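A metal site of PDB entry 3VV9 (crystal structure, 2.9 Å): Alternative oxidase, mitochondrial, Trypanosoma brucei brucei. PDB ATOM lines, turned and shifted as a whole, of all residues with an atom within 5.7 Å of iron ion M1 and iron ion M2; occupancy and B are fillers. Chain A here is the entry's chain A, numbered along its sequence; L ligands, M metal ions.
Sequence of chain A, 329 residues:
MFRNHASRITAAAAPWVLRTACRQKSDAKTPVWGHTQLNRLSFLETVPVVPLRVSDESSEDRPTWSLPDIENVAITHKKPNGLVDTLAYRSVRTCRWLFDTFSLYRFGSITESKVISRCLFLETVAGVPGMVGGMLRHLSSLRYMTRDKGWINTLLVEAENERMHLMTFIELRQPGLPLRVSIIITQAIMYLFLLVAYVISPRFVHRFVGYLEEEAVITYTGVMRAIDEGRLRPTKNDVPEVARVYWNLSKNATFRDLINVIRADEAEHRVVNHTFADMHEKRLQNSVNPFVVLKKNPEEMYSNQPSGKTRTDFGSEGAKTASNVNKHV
Of the 12 residues printed, 3 come within 4 Å of iron ion M1. Along chain A the residues within 4 Å of iron ion M1 span positions 162 to 266. The nearest printed residue that does not touch iron ion M1 is His 269 (4.4 Å).
Iron ion M1 is bound by OE2 of Glu 266 (2.1 Å), OE2 of Glu 213 (2.3 Å), OE2 of Glu 162 (2.3 Å) and OE1 of Glu 213 (2.5 Å).
Iron ion M2 is bound by the side-chain carboxylate (OE1) of Glu 266, the side-chain carboxylate (OE1) of Glu 123, an oxygen (O1) of the ligand, the side-chain carboxylate (OE2) of Glu 123 and the side-chain carboxylate (OE1) of Glu 162.
OE2 of Glu 123 lies close to ND1 of His 165 (2.9 Å). A ring nitrogen (ND1) of His 165 sits close to the side-chain carboxylate (OE1) of Glu 162. OE2 of Glu 213 lies close to ND1 of His 269. The side-chain hydroxyl (OH) of Tyr 220 sits close to the side-chain carboxylate (OE1) of Glu 123. OE2 of Glu 162 lies close to ND1 of His 269 (3.0 Å). OE1 of Glu 266 lies close to ND1 of His 165 (3.3 Å). N of Glu 266 sits close to ND1 of His 269, 3.5 Å away.
Ala 126 touches iron ion M2 (CB to FE, 3.7 Å). ND1 of His 165 touches iron ion M2, 3.3 Å away. Within 4 Å of iron ion M2: Glu 123, Ala 126, Glu 162, His 165 and Glu 266. The nearest printed residue that does not touch iron ion M2 is Tyr 220 (4.01 Å).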
ATOM      1  N   GLU A 123     -22.439 -15.934 -18.525  1.00  0.00           N
ATOM      2  CA  GLU A 123     -21.533 -16.228 -17.434  1.00  0.00           C
ATOM      3  C   GLU A 123     -20.681 -17.494 -17.649  1.00  0.00           C
ATOM      4  O   GLU A 123     -19.599 -17.646 -17.058  1.00  0.00           O
ATOM      5  CB  GLU A 123     -22.302 -16.266 -16.114  1.00  0.00           C
ATOM      6  CG  GLU A 123     -23.131 -15.009 -15.827  1.00  0.00           C
ATOM      7  CD  GLU A 123     -22.280 -13.777 -15.614  1.00  0.00           C
ATOM      8  OE1 GLU A 123     -22.351 -12.870 -16.472  1.00  0.00           O
ATOM      9  OE2 GLU A 123     -21.522 -13.692 -14.613  1.00  0.00           O
ATOM     10  N   ALA A 126     -18.193 -15.856 -19.420  1.00  0.00           N
ATOM     11  CA  ALA A 126     -17.748 -14.729 -18.551  1.00  0.00           C
ATOM     12  C   ALA A 126     -16.541 -14.976 -17.667  1.00  0.00           C
ATOM     13  O   ALA A 126     -15.796 -14.044 -17.376  1.00  0.00           O
ATOM     14  CB  ALA A 126     -18.905 -14.228 -17.696  1.00  0.00           C
ATOM     15  N   GLU A 158     -11.344 -12.647 -11.121  1.00  0.00           N
ATOM     16  CA  GLU A 158     -12.360 -12.392 -12.198  1.00  0.00           C
ATOM     17  C   GLU A 158     -12.968 -13.704 -12.684  1.00  0.00           C
ATOM     18  O   GLU A 158     -14.192 -13.799 -12.868  1.00  0.00           O
ATOM     19  CB  GLU A 158     -11.844 -11.591 -13.432  1.00  0.00           C
ATOM     20  CG  GLU A 158     -12.280 -12.203 -14.793  1.00  0.00           C
ATOM     21  CD  GLU A 158     -12.365 -11.247 -16.011  1.00  0.00           C
ATOM     22  OE1 GLU A 158     -11.323 -10.655 -16.411  1.00  0.00           O
ATOM     23  OE2 GLU A 158     -13.475 -11.124 -16.619  1.00  0.00           O
ATOM     24  N   GLU A 162     -16.885 -14.440 -11.580  1.00  0.00           N
ATOM     25  CA  GLU A 162     -17.949 -14.728 -12.549  1.00  0.00           C
ATOM     26  C   GLU A 162     -18.418 -16.187 -12.372  1.00  0.00           C
ATOM     27  O   GLU A 162     -19.622 -16.456 -12.387  1.00  0.00           O
ATOM     28  CB  GLU A 162     -17.538 -14.438 -14.009  1.00  0.00           C
ATOM     29  CG  GLU A 162     -16.876 -13.069 -14.262  1.00  0.00           C
ATOM     30  CD  GLU A 162     -17.814 -11.848 -14.265  1.00  0.00           C
ATOM     31  OE1 GLU A 162     -18.988 -11.973 -13.860  1.00  0.00           O
ATOM     32  OE2 GLU A 162     -17.347 -10.733 -14.665  1.00  0.00           O
ATOM     33  N   HIS A 165     -21.016 -15.731  -9.928  1.00  0.00           N
ATOM     34  CA  HIS A 165     -22.164 -15.231 -10.708  1.00  0.00           C
ATOM     35  C   HIS A 165     -22.976 -16.395 -11.324  1.00  0.00           C
ATOM     36  O   HIS A 165     -24.202 -16.371 -11.349  1.00  0.00           O
ATOM     37  CB  HIS A 165     -21.688 -14.352 -11.873  1.00  0.00           C
ATOM     38  CG  HIS A 165     -21.244 -12.975 -11.485  1.00  0.00           C
ATOM     39  ND1 HIS A 165     -21.351 -11.897 -12.353  1.00  0.00           N
ATOM     40  CD2 HIS A 165     -20.730 -12.490 -10.339  1.00  0.00           C
ATOM     41  CE1 HIS A 165     -20.918 -10.815 -11.746  1.00  0.00           C
ATOM     42  NE2 HIS A 165     -20.527 -11.147 -10.528  1.00  0.00           N
ATOM     43  N   LEU A 212     -16.727  -6.058 -23.158  1.00  0.00           N
ATOM     44  CA  LEU A 212     -17.772  -6.984 -22.685  1.00  0.00           C
ATOM     45  C   LEU A 212     -18.276  -6.593 -21.296  1.00  0.00           C
ATOM     46  O   LEU A 212     -19.425  -6.845 -20.978  1.00  0.00           O
ATOM     47  CB  LEU A 212     -17.300  -8.428 -22.659  1.00  0.00           C
ATOM     48  CG  LEU A 212     -17.091  -9.234 -23.955  1.00  0.00           C
ATOM     49  CD1 LEU A 212     -16.668 -10.689 -23.650  1.00  0.00           C
ATOM     50  CD2 LEU A 212     -18.341  -9.194 -24.822  1.00  0.00           C
ATOM     51  N   GLU A 213     -17.421  -5.970 -20.482  1.00  0.00           N
ATOM     52  CA  GLU A 213     -17.880  -5.430 -19.198  1.00  0.00           C
ATOM     53  C   GLU A 213     -18.834  -4.234 -19.318  1.00  0.00           C
ATOM     54  O   GLU A 213     -19.992  -4.321 -18.886  1.00  0.00           O
ATOM     55  CB  GLU A 213     -16.708  -5.158 -18.282  1.00  0.00           C
ATOM     56  CG  GLU A 213     -16.040  -6.432 -17.795  1.00  0.00           C
ATOM     57  CD  GLU A 213     -17.033  -7.441 -17.217  1.00  0.00           C
ATOM     58  OE1 GLU A 213     -18.168  -7.571 -17.764  1.00  0.00           O
ATOM     59  OE2 GLU A 213     -16.673  -8.136 -16.228  1.00  0.00           O
ATOM     60  N   ALA A 216     -21.933  -5.498 -19.867  1.00  0.00           N
ATOM     61  CA  ALA A 216     -22.409  -6.190 -18.675  1.00  0.00           C
ATOM     62  C   ALA A 216     -23.073  -5.187 -17.740  1.00  0.00           C
ATOM     63  O   ALA A 216     -24.200  -5.431 -17.256  1.00  0.00           O
ATOM     64  CB  ALA A 216     -21.275  -6.892 -17.967  1.00  0.00           C
ATOM     65  N   TYR A 220     -27.230  -5.254 -17.028  1.00  0.00           N
ATOM     66  CA  TYR A 220     -27.754  -5.265 -15.659  1.00  0.00           C
ATOM     67  C   TYR A 220     -28.358  -3.944 -15.230  1.00  0.00           C
ATOM     68  O   TYR A 220     -29.360  -3.911 -14.510  1.00  0.00           O
ATOM     69  CB  TYR A 220     -26.674  -5.669 -14.649  1.00  0.00           C
ATOM     70  CG  TYR A 220     -26.166  -7.087 -14.787  1.00  0.00           C
ATOM     71  CD1 TYR A 220     -27.023  -8.180 -14.706  1.00  0.00           C
ATOM     72  CD2 TYR A 220     -24.797  -7.346 -14.976  1.00  0.00           C
ATOM     73  CE1 TYR A 220     -26.552  -9.480 -14.831  1.00  0.00           C
ATOM     74  CE2 TYR A 220     -24.315  -8.644 -15.109  1.00  0.00           C
ATOM     75  CZ  TYR A 220     -25.192  -9.707 -15.036  1.00  0.00           C
ATOM     76  OH  TYR A 220     -24.714 -10.969 -15.144  1.00  0.00           O
ATOM     77  N   ILE A 262     -23.776  -7.899  -8.489  1.00  0.00           N
ATOM     78  CA  ILE A 262     -23.453  -8.527  -9.789  1.00  0.00           C
ATOM     79  C   ILE A 262     -23.032  -7.459 -10.799  1.00  0.00           C
ATOM     80  O   ILE A 262     -22.113  -7.676 -11.614  1.00  0.00           O
ATOM     81  CB  ILE A 262     -24.611  -9.377 -10.402  1.00  0.00           C
ATOM     82  CG1 ILE A 262     -24.735 -10.746  -9.711  1.00  0.00           C
ATOM     83  CG2 ILE A 262     -24.366  -9.672 -11.863  1.00  0.00           C
ATOM     84  CD1 ILE A 262     -25.745 -11.663 -10.361  1.00  0.00           C
ATOM     85  N   GLU A 266     -19.053  -6.649 -12.048  1.00  0.00           N
ATOM     86  CA  GLU A 266     -18.797  -6.385 -13.457  1.00  0.00           C
ATOM     87  C   GLU A 266     -18.074  -5.054 -13.699  1.00  0.00           C
ATOM     88  O   GLU A 266     -16.990  -5.023 -14.269  1.00  0.00           O
ATOM     89  CB  GLU A 266     -20.087  -6.421 -14.299  1.00  0.00           C
ATOM     90  CG  GLU A 266     -20.828  -7.749 -14.363  1.00  0.00           C
ATOM     91  CD  GLU A 266     -19.942  -8.928 -14.755  1.00  0.00           C
ATOM     92  OE1 GLU A 266     -20.500 -10.016 -14.938  1.00  0.00           O
ATOM     93  OE2 GLU A 266     -18.708  -8.769 -14.875  1.00  0.00           O
ATOM     94  N   HIS A 269     -14.448  -5.187 -12.999  1.00  0.00           N
ATOM     95  CA  HIS A 269     -13.821  -5.928 -14.082  1.00  0.00           C
ATOM     96  C   HIS A 269     -13.592  -5.024 -15.308  1.00  0.00           C
ATOM     97  O   HIS A 269     -12.537  -5.085 -15.945  1.00  0.00           O
ATOM     98  CB  HIS A 269     -14.640  -7.164 -14.405  1.00  0.00           C
ATOM     99  CG  HIS A 269     -14.959  -8.009 -13.209  1.00  0.00           C
ATOM    100  ND1 HIS A 269     -16.224  -8.493 -12.947  1.00  0.00           N
ATOM    101  CD2 HIS A 269     -14.172  -8.442 -12.181  1.00  0.00           C
ATOM    102  CE1 HIS A 269     -16.200  -9.187 -11.818  1.00  0.00           C
ATOM    103  NE2 HIS A 269     -14.972  -9.174 -11.341  1.00  0.00           N
HETATM  104  O1  LIG L   1     -21.699 -10.785 -17.219  1.00  0.00           O
HETATM  105 FE    FE M   1     -18.166  -9.822 -16.652  1.00  0.00          FE
HETATM  106 FE    FE M   2     -20.827 -11.846 -15.584  1.00  0.00          FE
